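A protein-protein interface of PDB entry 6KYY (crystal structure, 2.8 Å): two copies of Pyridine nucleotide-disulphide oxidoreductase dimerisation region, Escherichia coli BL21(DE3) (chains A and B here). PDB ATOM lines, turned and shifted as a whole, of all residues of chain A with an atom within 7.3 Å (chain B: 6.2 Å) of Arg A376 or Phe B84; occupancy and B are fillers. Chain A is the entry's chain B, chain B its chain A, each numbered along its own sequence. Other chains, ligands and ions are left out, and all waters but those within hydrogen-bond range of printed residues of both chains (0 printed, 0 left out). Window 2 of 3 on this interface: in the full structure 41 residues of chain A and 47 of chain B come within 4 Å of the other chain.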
ATOM      1  N   VAL A 369      14.292  15.934  -6.613  1.00  0.00           N
ATOM      2  CA  VAL A 369      15.407  16.679  -6.039  1.00  0.00           C
ATOM      3  C   VAL A 369      15.478  16.463  -4.532  1.00  0.00           C
ATOM      4  O   VAL A 369      16.561  16.526  -3.936  1.00  0.00           O
ATOM      5  CB  VAL A 369      15.285  18.168  -6.422  1.00  0.00           C
ATOM      6  CG1 VAL A 369      16.049  19.058  -5.459  1.00  0.00           C
ATOM      7  CG2 VAL A 369      15.784  18.379  -7.843  1.00  0.00           C
ATOM      8  N   ALA A 370      14.342  16.154  -3.897  1.00  0.00           N
ATOM      9  CA  ALA A 370      14.333  15.826  -2.476  1.00  0.00           C
ATOM     10  C   ALA A 370      15.276  14.678  -2.135  1.00  0.00           C
ATOM     11  O   ALA A 370      15.601  14.484  -0.958  1.00  0.00           O
ATOM     12  CB  ALA A 370      12.911  15.478  -2.029  1.00  0.00           C
ATOM     13  N   ALA A 371      15.722  13.917  -3.132  1.00  0.00           N
ATOM     14  CA  ALA A 371      16.671  12.831  -2.934  1.00  0.00           C
ATOM     15  C   ALA A 371      18.120  13.257  -3.134  1.00  0.00           C
ATOM     16  O   ALA A 371      19.015  12.411  -3.049  1.00  0.00           O
ATOM     17  CB  ALA A 371      16.345  11.671  -3.880  1.00  0.00           C
ATOM     18  N   ILE A 372      18.376  14.536  -3.400  1.00  0.00           N
ATOM     19  CA  ILE A 372      19.729  15.046  -3.605  1.00  0.00           C
ATOM     20  C   ILE A 372      20.175  15.713  -2.306  1.00  0.00           C
ATOM     21  O   ILE A 372      19.687  16.811  -1.989  1.00  0.00           O
ATOM     22  CB  ILE A 372      19.792  16.026  -4.782  1.00  0.00           C
ATOM     23  CG1 ILE A 372      19.157  15.405  -6.028  1.00  0.00           C
ATOM     24  CG2 ILE A 372      21.232  16.431  -5.060  1.00  0.00           C
ATOM     25  CD1 ILE A 372      19.250  16.278  -7.260  1.00  0.00           C
ATOM     26  N   PRO A 373      21.086  15.107  -1.538  1.00  0.00           N
ATOM     27  CA  PRO A 373      21.438  15.679  -0.227  1.00  0.00           C
ATOM     28  C   PRO A 373      22.011  17.083  -0.299  1.00  0.00           C
ATOM     29  O   PRO A 373      21.854  17.851   0.658  1.00  0.00           O
ATOM     30  CB  PRO A 373      22.467  14.679   0.320  1.00  0.00           C
ATOM     31  CG  PRO A 373      22.161  13.399  -0.389  1.00  0.00           C
ATOM     32  CD  PRO A 373      21.738  13.808  -1.768  1.00  0.00           C
ATOM     33  N   ARG A 374      22.667  17.451  -1.402  1.00  0.00           N
ATOM     34  CA  ARG A 374      23.210  18.801  -1.512  1.00  0.00           C
ATOM     35  C   ARG A 374      22.104  19.840  -1.654  1.00  0.00           C
ATOM     36  O   ARG A 374      22.274  20.988  -1.226  1.00  0.00           O
ATOM     37  CB  ARG A 374      24.181  18.882  -2.689  1.00  0.00           C
ATOM     38  CG  ARG A 374      24.776  20.262  -2.909  1.00  0.00           C
ATOM     39  CD  ARG A 374      25.987  20.500  -2.017  1.00  0.00           C
ATOM     40  NE  ARG A 374      26.124  21.896  -1.606  1.00  0.00           N
ATOM     41  CZ  ARG A 374      26.371  22.909  -2.433  1.00  0.00           C
ATOM     42  NH1 ARG A 374      26.479  24.141  -1.957  1.00  0.00           N
ATOM     43  NH2 ARG A 374      26.511  22.695  -3.734  1.00  0.00           N
ATOM     44  N   ALA A 375      20.968  19.464  -2.247  1.00  0.00           N
ATOM     45  CA  ALA A 375      19.834  20.378  -2.301  1.00  0.00           C
ATOM     46  C   ALA A 375      19.287  20.668  -0.912  1.00  0.00           C
ATOM     47  O   ALA A 375      18.812  21.779  -0.652  1.00  0.00           O
ATOM     48  CB  ALA A 375      18.738  19.805  -3.196  1.00  0.00           C
ATOM     49  N   ARG A 376      19.344  19.687  -0.008  1.00  0.00           N
ATOM     50  CA  ARG A 376      18.979  19.940   1.381  1.00  0.00           C
ATOM     51  C   ARG A 376      20.031  20.785   2.086  1.00  0.00           C
ATOM     52  O   ARG A 376      19.695  21.581   2.971  1.00  0.00           O
ATOM     53  CB  ARG A 376      18.778  18.621   2.122  1.00  0.00           C
ATOM     54  CG  ARG A 376      17.505  18.564   2.941  1.00  0.00           C
ATOM     55  CD  ARG A 376      17.141  17.130   3.274  1.00  0.00           C
ATOM     56  NE  ARG A 376      16.288  16.537   2.250  1.00  0.00           N
ATOM     57  CZ  ARG A 376      14.970  16.701   2.189  1.00  0.00           C
ATOM     58  NH1 ARG A 376      14.349  17.438   3.099  1.00  0.00           N
ATOM     59  NH2 ARG A 376      14.273  16.120   1.222  1.00  0.00           N
ATOM     60  N   VAL A 377      21.302  20.625   1.710  1.00  0.00           N
ATOM     61  CA  VAL A 377      22.373  21.440   2.271  1.00  0.00           C
ATOM     62  C   VAL A 377      22.163  22.917   1.961  1.00  0.00           C
ATOM     63  O   VAL A 377      22.633  23.782   2.710  1.00  0.00           O
ATOM     64  CB  VAL A 377      23.735  20.923   1.747  1.00  0.00           C
ATOM     65  CG1 VAL A 377      24.872  21.860   2.116  1.00  0.00           C
ATOM     66  CG2 VAL A 377      24.013  19.526   2.284  1.00  0.00           C
ATOM     67  N   MET A 378      21.433  23.234   0.891  1.00  0.00           N
ATOM     68  CA  MET A 378      21.218  24.610   0.466  1.00  0.00           C
ATOM     69  C   MET A 378      19.805  25.109   0.748  1.00  0.00           C
ATOM     70  O   MET A 378      19.444  26.198   0.287  1.00  0.00           O
ATOM     71  CB  MET A 378      21.538  24.750  -1.023  1.00  0.00           C
ATOM     72  CG  MET A 378      22.948  24.323  -1.386  1.00  0.00           C
ATOM     73  SD  MET A 378      23.518  25.042  -2.935  1.00  0.00           S
ATOM     74  CE  MET A 378      23.050  23.759  -4.090  1.00  0.00           C
ATOM     75  N   ASN A 379      18.999  24.342   1.486  1.00  0.00           N
ATOM     76  CA  ASN A 379      17.636  24.737   1.859  1.00  0.00           C
ATOM     77  C   ASN A 379      16.771  25.034   0.632  1.00  0.00           C
ATOM     78  O   ASN A 379      16.071  26.047   0.577  1.00  0.00           O
ATOM     79  CB  ASN A 379      17.648  25.937   2.814  1.00  0.00           C
ATOM     80  CG  ASN A 379      16.324  26.123   3.540  1.00  0.00           C
ATOM     81  OD1 ASN A 379      15.434  25.277   3.457  1.00  0.00           O
ATOM     82  ND2 ASN A 379      16.191  27.233   4.257  1.00  0.00           N
ATOM     83  N   ASP A 380      16.815  24.141  -0.369  1.00  0.00           N
ATOM     84  CA  ASP A 380      15.951  24.278  -1.552  1.00  0.00           C
ATOM     85  C   ASP A 380      15.862  22.903  -2.223  1.00  0.00           C
ATOM     86  O   ASP A 380      16.508  22.616  -3.233  1.00  0.00           O
ATOM     87  CB  ASP A 380      16.446  25.343  -2.530  1.00  0.00           C
ATOM     88  CG  ASP A 380      15.337  25.856  -3.439  1.00  0.00           C
ATOM     89  OD1 ASP A 380      15.534  26.867  -4.150  1.00  0.00           O
ATOM     90  OD2 ASP A 380      14.253  25.239  -3.436  1.00  0.00           O
ATOM     91  N   THR A 381      15.041  22.034  -1.635  1.00  0.00           N
ATOM     92  CA  THR A 381      14.815  20.696  -2.162  1.00  0.00           C
ATOM     93  C   THR A 381      13.668  20.650  -3.161  1.00  0.00           C
ATOM     94  O   THR A 381      13.009  19.611  -3.294  1.00  0.00           O
ATOM     95  CB  THR A 381      14.562  19.713  -1.014  1.00  0.00           C
ATOM     96  OG1 THR A 381      13.166  19.698  -0.694  1.00  0.00           O
ATOM     97  CG2 THR A 381      15.360  20.118   0.224  1.00  0.00           C
ATOM     98  N   VAL A 404      18.530  23.495  -8.019  1.00  0.00           N
ATOM     99  CA  VAL A 404      19.479  24.553  -7.710  1.00  0.00           C
ATOM    100  C   VAL A 404      20.796  24.250  -8.411  1.00  0.00           C
ATOM    101  O   VAL A 404      21.225  23.090  -8.490  1.00  0.00           O
ATOM    102  CB  VAL A 404      19.666  24.687  -6.189  1.00  0.00           C
ATOM    103  CG1 VAL A 404      18.547  25.526  -5.592  1.00  0.00           C
ATOM    104  CG2 VAL A 404      19.709  23.314  -5.541  1.00  0.00           C
ATOM    105  N   MET A 436      25.676  19.062  -6.553  1.00  0.00           N
ATOM    106  CA  MET A 436      24.474  18.780  -7.321  1.00  0.00           C
ATOM    107  C   MET A 436      24.783  18.015  -8.598  1.00  0.00           C
ATOM    108  O   MET A 436      23.917  17.296  -9.109  1.00  0.00           O
ATOM    109  CB  MET A 436      23.745  20.083  -7.655  1.00  0.00           C
ATOM    110  CG  MET A 436      23.352  20.904  -6.447  1.00  0.00           C
ATOM    111  SD  MET A 436      22.154  20.045  -5.418  1.00  0.00           S
ATOM    112  CE  MET A 436      20.788  19.872  -6.557  1.00  0.00           C
ATOM    113  N   THR B  60      26.165  22.028   5.451  1.00  0.00           N
ATOM    114  CA  THR B  60      24.895  22.677   5.766  1.00  0.00           C
ATOM    115  C   THR B  60      25.129  23.943   6.578  1.00  0.00           C
ATOM    116  O   THR B  60      24.432  24.949   6.395  1.00  0.00           O
ATOM    117  CB  THR B  60      23.977  21.718   6.525  1.00  0.00           C
ATOM    118  OG1 THR B  60      23.755  20.540   5.738  1.00  0.00           O
ATOM    119  CG2 THR B  60      22.640  22.378   6.825  1.00  0.00           C
ATOM    120  N   ARG B  77      19.024  24.230  12.328  1.00  0.00           N
ATOM    121  CA  ARG B  77      18.663  23.737  11.003  1.00  0.00           C
ATOM    122  C   ARG B  77      19.542  22.565  10.582  1.00  0.00           C
ATOM    123  O   ARG B  77      19.069  21.646   9.904  1.00  0.00           O
ATOM    124  CB  ARG B  77      18.752  24.867   9.980  1.00  0.00           C
ATOM    125  CG  ARG B  77      18.245  24.485   8.602  1.00  0.00           C
ATOM    126  CD  ARG B  77      18.916  25.313   7.523  1.00  0.00           C
ATOM    127  NE  ARG B  77      18.993  24.597   6.254  1.00  0.00           N
ATOM    128  CZ  ARG B  77      20.061  24.594   5.464  1.00  0.00           C
ATOM    129  NH1 ARG B  77      21.148  25.270   5.813  1.00  0.00           N
ATOM    130  NH2 ARG B  77      20.044  23.914   4.327  1.00  0.00           N
ATOM    131  N   ASN B  79      20.471  20.398  12.600  1.00  0.00           N
ATOM    132  CA  ASN B  79      19.930  19.274  13.354  1.00  0.00           C
ATOM    133  C   ASN B  79      18.756  18.620  12.636  1.00  0.00           C
ATOM    134  O   ASN B  79      18.575  17.402  12.745  1.00  0.00           O
ATOM    135  CB  ASN B  79      19.516  19.734  14.752  1.00  0.00           C
ATOM    136  CG  ASN B  79      20.701  19.895  15.684  1.00  0.00           C
ATOM    137  OD1 ASN B  79      21.683  19.157  15.592  1.00  0.00           O
ATOM    138  ND2 ASN B  79      20.617  20.863  16.589  1.00  0.00           N
ATOM    139  N   GLU B  80      17.953  19.391  11.898  1.00  0.00           N
ATOM    140  CA  GLU B  80      16.822  18.799  11.194  1.00  0.00           C
ATOM    141  C   GLU B  80      17.185  18.261   9.816  1.00  0.00           C
ATOM    142  O   GLU B  80      16.449  17.419   9.289  1.00  0.00           O
ATOM    143  CB  GLU B  80      15.664  19.802  11.067  1.00  0.00           C
ATOM    144  CG  GLU B  80      16.046  21.225  10.708  1.00  0.00           C
ATOM    145  CD  GLU B  80      14.835  22.076  10.357  1.00  0.00           C
ATOM    146  OE1 GLU B  80      14.832  23.282  10.683  1.00  0.00           O
ATOM    147  OE2 GLU B  80      13.883  21.535   9.756  1.00  0.00           O
ATOM    148  N   VAL B  81      18.294  18.705   9.221  1.00  0.00           N
ATOM    149  CA  VAL B  81      18.708  18.114   7.951  1.00  0.00           C
ATOM    150  C   VAL B  81      19.433  16.791   8.181  1.00  0.00           C
ATOM    151  O   VAL B  81      19.359  15.884   7.343  1.00  0.00           O
ATOM    152  CB  VAL B  81      19.570  19.097   7.136  1.00  0.00           C
ATOM    153  CG1 VAL B  81      20.874  19.394   7.848  1.00  0.00           C
ATOM    154  CG2 VAL B  81      19.841  18.541   5.745  1.00  0.00           C
ATOM    155  N   VAL B  82      20.124  16.644   9.312  1.00  0.00           N
ATOM    156  CA  VAL B  82      20.765  15.370   9.608  1.00  0.00           C
ATOM    157  C   VAL B  82      19.763  14.390  10.206  1.00  0.00           C
ATOM    158  O   VAL B  82      19.860  13.180   9.972  1.00  0.00           O
ATOM    159  CB  VAL B  82      21.975  15.589  10.532  1.00  0.00           C
ATOM    160  CG1 VAL B  82      22.576  14.265  10.944  1.00  0.00           C
ATOM    161  CG2 VAL B  82      23.013  16.437   9.828  1.00  0.00           C
ATOM    162  N   ASN B  83      18.775  14.884  10.956  1.00  0.00           N
ATOM    163  CA  ASN B  83      17.747  13.991  11.483  1.00  0.00           C
ATOM    164  C   ASN B  83      16.894  13.409  10.363  1.00  0.00           C
ATOM    165  O   ASN B  83      16.541  12.224  10.398  1.00  0.00           O
ATOM    166  CB  ASN B  83      16.868  14.726  12.495  1.00  0.00           C
ATOM    167  CG  ASN B  83      15.819  13.823  13.113  1.00  0.00           C
ATOM    168  OD1 ASN B  83      16.137  12.934  13.903  1.00  0.00           O
ATOM    169  ND2 ASN B  83      14.561  14.038  12.748  1.00  0.00           N
ATOM    170  N   PHE B  84      16.551  14.225   9.361  1.00  0.00           N
ATOM    171  CA  PHE B  84      15.794  13.708   8.226  1.00  0.00           C
ATOM    172  C   PHE B  84      16.592  12.657   7.467  1.00  0.00           C
ATOM    173  O   PHE B  84      16.052  11.612   7.084  1.00  0.00           O
ATOM    174  CB  PHE B  84      15.393  14.847   7.285  1.00  0.00           C
ATOM    175  CG  PHE B  84      14.955  14.379   5.922  1.00  0.00           C
ATOM    176  CD1 PHE B  84      13.635  14.027   5.688  1.00  0.00           C
ATOM    177  CD2 PHE B  84      15.862  14.284   4.877  1.00  0.00           C
ATOM    178  CE1 PHE B  84      13.229  13.593   4.440  1.00  0.00           C
ATOM    179  CE2 PHE B  84      15.462  13.841   3.631  1.00  0.00           C
ATOM    180  CZ  PHE B  84      14.144  13.502   3.411  1.00  0.00           C
ATOM    181  N   LEU B  85      17.879  12.920   7.231  1.00  0.00           N
ATOM    182  CA  LEU B  85      18.693  11.989   6.460  1.00  0.00           C
ATOM    183  C   LEU B  85      19.035  10.740   7.262  1.00  0.00           C
ATOM    184  O   LEU B  85      19.212   9.663   6.683  1.00  0.00           O
ATOM    185  CB  LEU B  85      19.968  12.683   5.981  1.00  0.00           C
ATOM    186  CG  LEU B  85      19.816  13.648   4.803  1.00  0.00           C
ATOM    187  CD1 LEU B  85      21.157  14.260   4.440  1.00  0.00           C
ATOM    188  CD2 LEU B  85      19.205  12.940   3.604  1.00  0.00           C
ATOM    189  N   ARG B  86      19.135  10.863   8.587  1.00  0.00           N
ATOM    190  CA  ARG B  86      19.396   9.695   9.421  1.00  0.00           C
ATOM    191  C   ARG B  86      18.218   8.729   9.386  1.00  0.00           C
ATOM    192  O   ARG B  86      18.400   7.515   9.236  1.00  0.00           O
ATOM    193  CB  ARG B  86      19.700  10.136  10.853  1.00  0.00           C
ATOM    194  CG  ARG B  86      19.784   9.007  11.863  1.00  0.00           C
ATOM    195  CD  ARG B  86      20.012   9.556  13.260  1.00  0.00           C
ATOM    196  NE  ARG B  86      21.364  10.084  13.422  1.00  0.00           N
ATOM    197  CZ  ARG B  86      21.664  11.167  14.133  1.00  0.00           C
ATOM    198  NH1 ARG B  86      20.708  11.846  14.750  1.00  0.00           N
ATOM    199  NH2 ARG B  86      22.924  11.572  14.225  1.00  0.00           N
ATOM    200  N   ASN B  87      16.997   9.252   9.526  1.00  0.00           N
ATOM    201  CA  ASN B  87      15.811   8.415   9.375  1.00  0.00           C
ATOM    202  C   ASN B  87      15.697   7.879   7.955  1.00  0.00           C
ATOM    203  O   ASN B  87      15.292   6.729   7.746  1.00  0.00           O
ATOM    204  CB  ASN B  87      14.554   9.207   9.739  1.00  0.00           C
ATOM    205  CG  ASN B  87      14.423   9.447  11.228  1.00  0.00           C
ATOM    206  OD1 ASN B  87      15.209   8.934  12.025  1.00  0.00           O
ATOM    207  ND2 ASN B  87      13.422  10.232  11.613  1.00  0.00           N
ATOM    208  N   LYS B  88      16.053   8.702   6.966  1.00  0.00           N
ATOM    209  CA  LYS B  88      15.927   8.300   5.569  1.00  0.00           C
ATOM    210  C   LYS B  88      16.799   7.090   5.260  1.00  0.00           C
ATOM    211  O   LYS B  88      16.325   6.094   4.701  1.00  0.00           O
ATOM    212  CB  LYS B  88      16.292   9.473   4.658  1.00  0.00           C
ATOM    213  CG  LYS B  88      16.142   9.187   3.174  1.00  0.00           C
ATOM    214  CD  LYS B  88      14.853   9.775   2.628  1.00  0.00           C
ATOM    215  CE  LYS B  88      14.158   8.799   1.693  1.00  0.00           C
ATOM    216  NZ  LYS B  88      12.719   9.135   1.510  1.00  0.00           N
ATOM    217  N   ASN B  89      18.081   7.155   5.625  1.00  0.00           N
ATOM    218  CA  ASN B  89      19.004   6.085   5.266  1.00  0.00           C
ATOM    219  C   ASN B  89      18.689   4.788   6.002  1.00  0.00           C
ATOM    220  O   ASN B  89      18.924   3.701   5.461  1.00  0.00           O
ATOM    221  CB  ASN B  89      20.441   6.523   5.537  1.00  0.00           C
ATOM    222  CG  ASN B  89      21.069   7.216   4.345  1.00  0.00           C
ATOM    223  OD1 ASN B  89      21.494   6.568   3.391  1.00  0.00           O
ATOM    224  ND2 ASN B  89      21.122   8.542   4.390  1.00  0.00           N
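The guanidinium group (NH2) of Arg B77 sits at hydrogen-bond distance from the backbone carbonyl oxygen (O) of Val A377 (3.1 Å).
The guanidinium group of Arg B77 is in hydrogen-bond range of the backbone carbonyl oxygen of Arg A376, at 2.7 Å.
N of Asn A379 sits close to NH2 of Arg B77 (3.1 Å).
NH2 of Arg A376 sits at hydrogen-bond distance from O of Ala A370.
NH1 of Arg B77 lies within hydrogen-bond range of O of Thr B60 (3.4 Å).
NH1 of Arg A374 sits at hydrogen-bond distance from SD of Met A378 (3.2 Å).
Among the printed residues, merely in contact across the chains: Arg A376 with Val B81, Arg A376 with Phe B84, Val A377 with Thr B60 and Met A378 with Arg B77.
Arg A376 touches three residues of chain B.
Of the printed residues of chain B, Asn A379 touches Arg B77.
Printed residues of chain A within 4 Å of Arg B77: Arg A376, Val A377, Met A378 and Asn A379.
Printed residues of chain A within 4 Å of Val B81: Arg A376 (3.6 Å).
Of the printed residues of chain B, Val A377 touches Thr B60 and Arg B77.
Ala A370 touches none of the printed residues of chain B.
The nearest residue of chain A that does not touch Phe B84 is Ala A370 (4.6 Å).
The nearest printed residue of chain B that does not touch Asn A379 is Thr B60 (6.8 Å).
Of the 13 printed residues of chain B, 4 touch a printed residue of chain A.
Among the printed residues, 7 pairs touch across the chains.
No position is printed for both chains.
Of the 7 pairs that touch across the chains among the printed residues, none has its exchanged pair printed and touching as well.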
